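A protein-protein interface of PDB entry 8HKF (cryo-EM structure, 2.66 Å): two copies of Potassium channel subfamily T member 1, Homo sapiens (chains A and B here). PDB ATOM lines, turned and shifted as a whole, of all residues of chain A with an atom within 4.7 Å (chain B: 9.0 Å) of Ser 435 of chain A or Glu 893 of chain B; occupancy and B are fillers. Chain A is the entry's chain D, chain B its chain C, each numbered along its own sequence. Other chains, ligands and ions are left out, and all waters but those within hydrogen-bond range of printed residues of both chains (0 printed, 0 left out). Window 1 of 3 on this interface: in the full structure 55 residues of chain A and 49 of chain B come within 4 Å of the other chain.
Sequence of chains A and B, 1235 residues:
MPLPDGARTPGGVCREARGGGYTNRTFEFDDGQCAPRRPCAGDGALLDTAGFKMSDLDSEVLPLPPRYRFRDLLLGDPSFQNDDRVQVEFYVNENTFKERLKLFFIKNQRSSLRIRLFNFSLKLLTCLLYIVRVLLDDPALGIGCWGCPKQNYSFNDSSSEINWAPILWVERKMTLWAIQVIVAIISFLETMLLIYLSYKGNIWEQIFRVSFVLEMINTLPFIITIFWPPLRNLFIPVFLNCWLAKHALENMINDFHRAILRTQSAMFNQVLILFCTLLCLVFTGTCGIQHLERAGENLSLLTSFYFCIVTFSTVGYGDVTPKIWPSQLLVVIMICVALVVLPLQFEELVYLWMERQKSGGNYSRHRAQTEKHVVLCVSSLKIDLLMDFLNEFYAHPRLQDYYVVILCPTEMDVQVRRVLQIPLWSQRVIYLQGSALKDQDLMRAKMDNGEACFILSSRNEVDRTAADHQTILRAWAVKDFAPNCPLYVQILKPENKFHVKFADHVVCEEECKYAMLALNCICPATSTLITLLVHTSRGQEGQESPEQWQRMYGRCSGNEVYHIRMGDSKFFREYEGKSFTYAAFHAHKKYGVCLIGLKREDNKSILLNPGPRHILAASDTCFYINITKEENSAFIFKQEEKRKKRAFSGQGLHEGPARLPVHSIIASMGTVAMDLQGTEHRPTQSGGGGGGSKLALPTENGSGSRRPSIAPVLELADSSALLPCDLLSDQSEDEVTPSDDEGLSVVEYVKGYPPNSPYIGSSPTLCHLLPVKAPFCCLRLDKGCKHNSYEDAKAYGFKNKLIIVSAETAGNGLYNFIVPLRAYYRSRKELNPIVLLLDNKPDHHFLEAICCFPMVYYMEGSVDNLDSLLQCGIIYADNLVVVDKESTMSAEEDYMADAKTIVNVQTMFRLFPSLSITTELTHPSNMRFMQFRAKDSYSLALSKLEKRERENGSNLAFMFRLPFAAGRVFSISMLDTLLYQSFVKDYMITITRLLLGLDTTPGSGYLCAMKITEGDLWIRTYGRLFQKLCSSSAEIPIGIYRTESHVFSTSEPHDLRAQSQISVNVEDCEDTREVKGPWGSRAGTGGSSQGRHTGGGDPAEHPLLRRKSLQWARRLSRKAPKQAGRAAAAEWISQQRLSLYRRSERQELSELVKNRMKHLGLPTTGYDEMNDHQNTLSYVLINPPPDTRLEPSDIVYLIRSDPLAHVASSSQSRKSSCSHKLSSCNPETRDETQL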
ATOM      1  N   LEU A 407      28.229   6.775 -14.138  1.00  0.00           N
ATOM      2  CA  LEU A 407      26.784   6.604 -14.037  1.00  0.00           C
ATOM      3  C   LEU A 407      26.267   7.640 -13.047  1.00  0.00           C
ATOM      4  O   LEU A 407      26.370   7.459 -11.832  1.00  0.00           O
ATOM      5  CB  LEU A 407      26.449   5.181 -13.606  1.00  0.00           C
ATOM      6  CG  LEU A 407      24.987   4.751 -13.629  1.00  0.00           C
ATOM      7  CD1 LEU A 407      24.436   4.817 -15.039  1.00  0.00           C
ATOM      8  CD2 LEU A 407      24.880   3.345 -13.082  1.00  0.00           C
ATOM      9  N   PRO A 409      22.937  10.404 -12.249  1.00  0.00           N
ATOM     10  CA  PRO A 409      21.593  10.883 -12.620  1.00  0.00           C
ATOM     11  C   PRO A 409      21.571  12.315 -13.129  1.00  0.00           C
ATOM     12  O   PRO A 409      20.714  12.664 -13.951  1.00  0.00           O
ATOM     13  CB  PRO A 409      20.799  10.731 -11.314  1.00  0.00           C
ATOM     14  CG  PRO A 409      21.829  10.729 -10.237  1.00  0.00           C
ATOM     15  CD  PRO A 409      23.030  10.060 -10.820  1.00  0.00           C
ATOM     16  N   GLY A 434      21.941   8.231 -15.620  1.00  0.00           N
ATOM     17  CA  GLY A 434      21.090   7.139 -15.192  1.00  0.00           C
ATOM     18  C   GLY A 434      21.281   6.873 -13.719  1.00  0.00           C
ATOM     19  O   GLY A 434      22.024   7.574 -13.023  1.00  0.00           O
ATOM     20  N   SER A 435      20.600   5.834 -13.251  1.00  0.00           N
ATOM     21  CA  SER A 435      20.594   5.463 -11.847  1.00  0.00           C
ATOM     22  C   SER A 435      21.109   4.042 -11.683  1.00  0.00           C
ATOM     23  O   SER A 435      20.808   3.165 -12.498  1.00  0.00           O
ATOM     24  CB  SER A 435      19.186   5.568 -11.260  1.00  0.00           C
ATOM     25  OG  SER A 435      18.705   6.897 -11.329  1.00  0.00           O
ATOM     26  N   ALA A 436      21.893   3.819 -10.628  1.00  0.00           N
ATOM     27  CA  ALA A 436      22.261   2.457 -10.273  1.00  0.00           C
ATOM     28  C   ALA A 436      21.058   1.635  -9.838  1.00  0.00           C
ATOM     29  O   ALA A 436      21.130   0.403  -9.861  1.00  0.00           O
ATOM     30  CB  ALA A 436      23.313   2.465  -9.165  1.00  0.00           C
ATOM     31  N   LEU A 437      19.962   2.282  -9.455  1.00  0.00           N
ATOM     32  CA  LEU A 437      18.761   1.597  -9.005  1.00  0.00           C
ATOM     33  C   LEU A 437      17.871   1.152 -10.157  1.00  0.00           C
ATOM     34  O   LEU A 437      16.856   0.491  -9.917  1.00  0.00           O
ATOM     35  CB  LEU A 437      17.975   2.499  -8.048  1.00  0.00           C
ATOM     36  CG  LEU A 437      18.233   2.262  -6.558  1.00  0.00           C
ATOM     37  CD1 LEU A 437      19.696   2.473  -6.219  1.00  0.00           C
ATOM     38  CD2 LEU A 437      17.364   3.170  -5.714  1.00  0.00           C
ATOM     39  N   LYS A 438      18.221   1.505 -11.390  1.00  0.00           N
ATOM     40  CA  LYS A 438      17.556   1.000 -12.583  1.00  0.00           C
ATOM     41  C   LYS A 438      18.496   0.016 -13.263  1.00  0.00           C
ATOM     42  O   LYS A 438      19.595   0.393 -13.681  1.00  0.00           O
ATOM     43  CB  LYS A 438      17.191   2.138 -13.536  1.00  0.00           C
ATOM     44  CG  LYS A 438      16.517   3.313 -12.863  1.00  0.00           C
ATOM     45  CD  LYS A 438      15.139   3.552 -13.443  1.00  0.00           C
ATOM     46  CE  LYS A 438      14.839   5.034 -13.526  1.00  0.00           C
ATOM     47  NZ  LYS A 438      13.413   5.294 -13.862  1.00  0.00           N
ATOM     48  N   ASP A 441      19.881   1.047 -16.627  1.00  0.00           N
ATOM     49  CA  ASP A 441      21.050   1.917 -16.594  1.00  0.00           C
ATOM     50  C   ASP A 441      22.300   1.159 -16.174  1.00  0.00           C
ATOM     51  O   ASP A 441      23.415   1.564 -16.518  1.00  0.00           O
ATOM     52  CB  ASP A 441      20.798   3.096 -15.659  1.00  0.00           C
ATOM     53  CG  ASP A 441      19.663   3.975 -16.133  1.00  0.00           C
ATOM     54  OD1 ASP A 441      19.408   4.004 -17.354  1.00  0.00           O
ATOM     55  OD2 ASP A 441      19.023   4.634 -15.287  1.00  0.00           O
ATOM     56  N   LEU A 442      22.140   0.064 -15.428  1.00  0.00           N
ATOM     57  CA  LEU A 442      23.275  -0.797 -15.132  1.00  0.00           C
ATOM     58  C   LEU A 442      23.660  -1.664 -16.320  1.00  0.00           C
ATOM     59  O   LEU A 442      24.833  -2.032 -16.448  1.00  0.00           O
ATOM     60  CB  LEU A 442      22.971  -1.675 -13.920  1.00  0.00           C
ATOM     61  CG  LEU A 442      22.831  -0.926 -12.597  1.00  0.00           C
ATOM     62  CD1 LEU A 442      22.591  -1.898 -11.467  1.00  0.00           C
ATOM     63  CD2 LEU A 442      24.056  -0.098 -12.329  1.00  0.00           C
ATOM     64  N   ARG A 474      22.658   2.385  -3.614  1.00  0.00           N
ATOM     65  CA  ARG A 474      23.445   2.174  -4.824  1.00  0.00           C
ATOM     66  C   ARG A 474      24.330   0.943  -4.700  1.00  0.00           C
ATOM     67  O   ARG A 474      24.446   0.154  -5.644  1.00  0.00           O
ATOM     68  CB  ARG A 474      24.297   3.406  -5.114  1.00  0.00           C
ATOM     69  CG  ARG A 474      23.578   4.479  -5.886  1.00  0.00           C
ATOM     70  CD  ARG A 474      24.334   5.784  -5.822  1.00  0.00           C
ATOM     71  NE  ARG A 474      23.512   6.889  -6.291  1.00  0.00           N
ATOM     72  CZ  ARG A 474      23.573   8.123  -5.813  1.00  0.00           C
ATOM     73  NH1 ARG A 474      24.422   8.451  -4.854  1.00  0.00           N
ATOM     74  NH2 ARG A 474      22.757   9.050  -6.307  1.00  0.00           N
ATOM     75  N   LYS B 382       5.366  10.144 -14.707  1.00  0.00           N
ATOM     76  CA  LYS B 382       6.676   9.533 -14.564  1.00  0.00           C
ATOM     77  C   LYS B 382       6.660   8.157 -15.213  1.00  0.00           C
ATOM     78  O   LYS B 382       5.603   7.590 -15.500  1.00  0.00           O
ATOM     79  CB  LYS B 382       7.088   9.442 -13.090  1.00  0.00           C
ATOM     80  CG  LYS B 382       7.438  10.789 -12.476  1.00  0.00           C
ATOM     81  CD  LYS B 382       8.259  11.631 -13.442  1.00  0.00           C
ATOM     82  CE  LYS B 382       7.924  13.109 -13.319  1.00  0.00           C
ATOM     83  NZ  LYS B 382       8.044  13.810 -14.627  1.00  0.00           N
ATOM     84  N   GLN B 415      12.660  10.644 -19.468  1.00  0.00           N
ATOM     85  CA  GLN B 415      12.498   9.194 -19.471  1.00  0.00           C
ATOM     86  C   GLN B 415      11.207   8.785 -20.167  1.00  0.00           C
ATOM     87  O   GLN B 415      11.160   7.759 -20.855  1.00  0.00           O
ATOM     88  CB  GLN B 415      12.525   8.665 -18.040  1.00  0.00           C
ATOM     89  CG  GLN B 415      13.897   8.689 -17.402  1.00  0.00           C
ATOM     90  CD  GLN B 415      13.870   8.211 -15.969  1.00  0.00           C
ATOM     91  OE1 GLN B 415      13.766   7.014 -15.707  1.00  0.00           O
ATOM     92  NE2 GLN B 415      13.960   9.144 -15.029  1.00  0.00           N
ATOM     93  N   ARG B 418      11.677   8.930 -24.063  1.00  0.00           N
ATOM     94  CA  ARG B 418      12.388   7.819 -24.686  1.00  0.00           C
ATOM     95  C   ARG B 418      11.467   6.628 -24.914  1.00  0.00           C
ATOM     96  O   ARG B 418      11.539   5.967 -25.956  1.00  0.00           O
ATOM     97  CB  ARG B 418      13.585   7.417 -23.827  1.00  0.00           C
ATOM     98  CG  ARG B 418      14.665   8.478 -23.761  1.00  0.00           C
ATOM     99  CD  ARG B 418      15.756   8.098 -22.780  1.00  0.00           C
ATOM    100  NE  ARG B 418      16.599   9.238 -22.444  1.00  0.00           N
ATOM    101  CZ  ARG B 418      17.564   9.213 -21.535  1.00  0.00           C
ATOM    102  NH1 ARG B 418      17.837   8.116 -20.847  1.00  0.00           N
ATOM    103  NH2 ARG B 418      18.272  10.317 -21.310  1.00  0.00           N
ATOM    104  N   ALA B 891      12.536  13.242  -3.537  1.00  0.00           N
ATOM    105  CA  ALA B 891      13.836  13.041  -4.165  1.00  0.00           C
ATOM    106  C   ALA B 891      13.755  13.260  -5.672  1.00  0.00           C
ATOM    107  O   ALA B 891      12.725  12.990  -6.292  1.00  0.00           O
ATOM    108  CB  ALA B 891      14.364  11.648  -3.859  1.00  0.00           C
ATOM    109  N   GLU B 892      14.845  13.756  -6.257  1.00  0.00           N
ATOM    110  CA  GLU B 892      14.890  13.962  -7.701  1.00  0.00           C
ATOM    111  C   GLU B 892      14.987  12.631  -8.439  1.00  0.00           C
ATOM    112  O   GLU B 892      14.163  12.328  -9.308  1.00  0.00           O
ATOM    113  CB  GLU B 892      16.065  14.873  -8.064  1.00  0.00           C
ATOM    114  CG  GLU B 892      15.913  16.295  -7.551  1.00  0.00           C
ATOM    115  CD  GLU B 892      17.122  17.156  -7.852  1.00  0.00           C
ATOM    116  OE1 GLU B 892      18.153  16.602  -8.289  1.00  0.00           O
ATOM    117  OE2 GLU B 892      17.043  18.386  -7.652  1.00  0.00           O
ATOM    118  N   GLU B 893      15.990  11.825  -8.100  1.00  0.00           N
ATOM    119  CA  GLU B 893      16.056  10.457  -8.597  1.00  0.00           C
ATOM    120  C   GLU B 893      14.934   9.649  -7.956  1.00  0.00           C
ATOM    121  O   GLU B 893      14.868   9.533  -6.727  1.00  0.00           O
ATOM    122  CB  GLU B 893      17.425   9.856  -8.292  1.00  0.00           C
ATOM    123  CG  GLU B 893      17.507   8.346  -8.411  1.00  0.00           C
ATOM    124  CD  GLU B 893      18.927   7.837  -8.253  1.00  0.00           C
ATOM    125  OE1 GLU B 893      19.841   8.668  -8.073  1.00  0.00           O
ATOM    126  OE2 GLU B 893      19.130   6.607  -8.303  1.00  0.00           O
ATOM    127  N   ASP B 894      14.051   9.098  -8.790  1.00  0.00           N
ATOM    128  CA  ASP B 894      12.750   8.627  -8.316  1.00  0.00           C
ATOM    129  C   ASP B 894      12.883   7.479  -7.325  1.00  0.00           C
ATOM    130  O   ASP B 894      12.266   7.493  -6.253  1.00  0.00           O
ATOM    131  CB  ASP B 894      11.886   8.211  -9.506  1.00  0.00           C
ATOM    132  CG  ASP B 894      11.419   9.394 -10.327  1.00  0.00           C
ATOM    133  OD1 ASP B 894      11.517  10.536  -9.832  1.00  0.00           O
ATOM    134  OD2 ASP B 894      10.953   9.183 -11.465  1.00  0.00           O
ATOM    135  N   TYR B 895      13.688   6.471  -7.662  1.00  0.00           N
ATOM    136  CA  TYR B 895      13.753   5.270  -6.835  1.00  0.00           C
ATOM    137  C   TYR B 895      14.405   5.530  -5.483  1.00  0.00           C
ATOM    138  O   TYR B 895      14.332   4.672  -4.598  1.00  0.00           O
ATOM    139  CB  TYR B 895      14.505   4.162  -7.574  1.00  0.00           C
ATOM    140  CG  TYR B 895      13.762   3.596  -8.761  1.00  0.00           C
ATOM    141  CD1 TYR B 895      14.315   2.581  -9.526  1.00  0.00           C
ATOM    142  CD2 TYR B 895      12.505   4.068  -9.112  1.00  0.00           C
ATOM    143  CE1 TYR B 895      13.640   2.057 -10.610  1.00  0.00           C
ATOM    144  CE2 TYR B 895      11.825   3.555 -10.192  1.00  0.00           C
ATOM    145  CZ  TYR B 895      12.397   2.549 -10.937  1.00  0.00           C
ATOM    146  OH  TYR B 895      11.720   2.031 -12.017  1.00  0.00           O
ATOM    147  N   MET B 896      15.032   6.693  -5.301  1.00  0.00           N
ATOM    148  CA  MET B 896      15.663   7.021  -4.031  1.00  0.00           C
ATOM    149  C   MET B 896      14.669   7.495  -2.981  1.00  0.00           C
ATOM    150  O   MET B 896      15.078   7.760  -1.845  1.00  0.00           O
ATOM    151  CB  MET B 896      16.735   8.090  -4.236  1.00  0.00           C
ATOM    152  CG  MET B 896      18.062   7.546  -4.726  1.00  0.00           C
ATOM    153  SD  MET B 896      18.782   6.348  -3.589  1.00  0.00           S
ATOM    154  CE  MET B 896      20.077   5.664  -4.614  1.00  0.00           C
ATOM    155  N   ALA B 897      13.386   7.620  -3.328  1.00  0.00           N
ATOM    156  CA  ALA B 897      12.397   8.066  -2.353  1.00  0.00           C
ATOM    157  C   ALA B 897      12.258   7.082  -1.201  1.00  0.00           C
ATOM    158  O   ALA B 897      11.931   7.483  -0.078  1.00  0.00           O
ATOM    159  CB  ALA B 897      11.047   8.281  -3.034  1.00  0.00           C
ATOM    160  N   ASP B 898      12.501   5.799  -1.453  1.00  0.00           N
ATOM    161  CA  ASP B 898      12.407   4.769  -0.428  1.00  0.00           C
ATOM    162  C   ASP B 898      13.721   4.530   0.299  1.00  0.00           C
ATOM    163  O   ASP B 898      13.793   3.616   1.124  1.00  0.00           O
ATOM    164  CB  ASP B 898      11.926   3.452  -1.045  1.00  0.00           C
ATOM    165  CG  ASP B 898      10.643   3.610  -1.830  1.00  0.00           C
ATOM    166  OD1 ASP B 898       9.671   4.165  -1.277  1.00  0.00           O
ATOM    167  OD2 ASP B 898      10.602   3.174  -2.999  1.00  0.00           O
ATOM    168  N   ALA B 899      14.756   5.327   0.014  1.00  0.00           N
ATOM    169  CA  ALA B 899      16.079   5.051   0.567  1.00  0.00           C
ATOM    170  C   ALA B 899      16.074   5.108   2.090  1.00  0.00           C
ATOM    171  O   ALA B 899      16.680   4.256   2.751  1.00  0.00           O
ATOM    172  CB  ALA B 899      17.101   6.034  -0.002  1.00  0.00           C
ATOM    173  N   HIS B 923       7.938   2.195  -4.939  1.00  0.00           N
ATOM    174  CA  HIS B 923       8.310   1.543  -6.179  1.00  0.00           C
ATOM    175  C   HIS B 923       8.482   0.048  -5.956  1.00  0.00           C
ATOM    176  O   HIS B 923       9.224  -0.357  -5.049  1.00  0.00           O
ATOM    177  CB  HIS B 923       9.612   2.138  -6.733  1.00  0.00           C
ATOM    178  CG  HIS B 923       9.622   3.634  -6.772  1.00  0.00           C
ATOM    179  ND1 HIS B 923       8.924   4.359  -7.713  1.00  0.00           N
ATOM    180  CD2 HIS B 923      10.235   4.542  -5.976  1.00  0.00           C
ATOM    181  CE1 HIS B 923       9.113   5.649  -7.500  1.00  0.00           C
ATOM    182  NE2 HIS B 923       9.905   5.787  -6.453  1.00  0.00           N
ATOM    183  N   ASN B 926      12.022  -1.466  -5.714  1.00  0.00           N
ATOM    184  CA  ASN B 926      12.774  -1.373  -4.472  1.00  0.00           C
ATOM    185  C   ASN B 926      12.467  -2.505  -3.503  1.00  0.00           C
ATOM    186  O   ASN B 926      13.059  -2.547  -2.419  1.00  0.00           O
ATOM    187  CB  ASN B 926      12.495  -0.033  -3.792  1.00  0.00           C
ATOM    188  CG  ASN B 926      13.088   1.135  -4.549  1.00  0.00           C
ATOM    189  OD1 ASN B 926      14.009   0.968  -5.346  1.00  0.00           O
ATOM    190  ND2 ASN B 926      12.565   2.328  -4.299  1.00  0.00           N
ATOM    191  N   ARG B 928      13.300  -5.534  -3.574  1.00  0.00           N
ATOM    192  CA  ARG B 928      14.436  -6.422  -3.369  1.00  0.00           C
ATOM    193  C   ARG B 928      15.291  -5.997  -2.185  1.00  0.00           C
ATOM    194  O   ARG B 928      16.104  -6.793  -1.704  1.00  0.00           O
ATOM    195  CB  ARG B 928      15.294  -6.466  -4.630  1.00  0.00           C
ATOM    196  CG  ARG B 928      15.140  -5.228  -5.486  1.00  0.00           C
ATOM    197  CD  ARG B 928      16.317  -5.017  -6.410  1.00  0.00           C
ATOM    198  NE  ARG B 928      16.209  -3.744  -7.112  1.00  0.00           N
ATOM    199  CZ  ARG B 928      17.176  -3.203  -7.840  1.00  0.00           C
ATOM    200  NH1 ARG B 928      18.338  -3.813  -8.006  1.00  0.00           N
ATOM    201  NH2 ARG B 928      16.972  -2.022  -8.416  1.00  0.00           N
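Of the 15 printed residues of chain B, 5 touch a printed residue of chain A. Hydrophobic or aromatic side chains of chain B that line the printed part of chain A: Tyr 895 and Met 896. Along chain B the printed residues that touch a printed residue of chain A span positions 415 to 928. Printed residues of chain A that touch a printed residue of chain B: Pro 409, Ser 435, Leu 437, Lys 438 and Arg 474. Hydrophobic or aromatic side chains of chain A within 4 Å of the printed part of chain B: Pro 409 and Leu 437. Among the printed residues, 9 pairs touch across the chains. Among the printed residues, Asp or Glu carboxylates within 4 Å of a Lys or Arg side-chain nitrogen of the other chain: Arg 474 of chain A with Glu 893 of chain B.
Ser 435 of chain A touches one residue of chain B. No residue of chain B comes within 4 Å of Gly 434 of chain A. No residue of chain B comes within 4 Å of Ala 436 of chain A. Printed residues of chain A within 4 Å of Met 896 of chain B: Leu 437 and Arg 474. Of the printed residues of chain B, Arg 474 of chain A touches Glu 893 (3.4 Å) and Met 896 (3.9 Å). Of the printed residues of chain B, Pro 409 of chain A touches Glu 893 (3.6 Å). Of the printed residues of chain A, Gln 415 of chain B touches Lys 438 (2.5 Å). Ala 899 of chain B touches none of the printed residues of chain A. The nearest residue of chain B that does not touch Ser 435 of chain A is Asp 894 of chain B (5.7 Å).
Glu 893 of chain B touches Pro 409 of chain A (OE1 to CG, 3.6 Å). O of Leu 437 of chain A touches CD1 of Tyr 895 of chain B, at 3.3 Å. CE of Met 896 of chain B touches CD1 of Leu 437 of chain A, 3.6 Å away. Lys 438 of chain A touches Tyr 895 of chain B. Met 896 of chain B touches Arg 474 of chain A (CE to CG, 3.9 Å).
OE1 of Gln 415 of chain B sits at hydrogen-bond distance from NZ of Lys 438 of chain A, 2.5 Å away. The side-chain hydroxyl (OG) of Ser 435 of chain A lies within hydrogen-bond range of the side-chain carboxylate (OE2) of Glu 893 of chain B (3.1 Å). OE1 of Glu 893 of chain B lies within salt-bridge range of NH2 of Arg 474 of chain A (3.4 Å). The backbone carbonyl oxygen (O) of Leu 437 of chain A sits at hydrogen-bond distance from the guanidinium group (NH2) of Arg 928 of chain B, at 2.9 Å.
No position is printed for both chains. Of the 9 pairs that touch across the chains among the printed residues, none has its exchanged pair printed and touching as well.
O of Tyr 895 of chain B is in hydrogen-bond range of ND2 of Asn 926 of chain B, at 3.0 Å. The backbone NH (N) of Ser 435 of chain A is in hydrogen-bond range of the side-chain carboxylate (OD2) of Asp 441 of chain A, 2.8 Å away.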
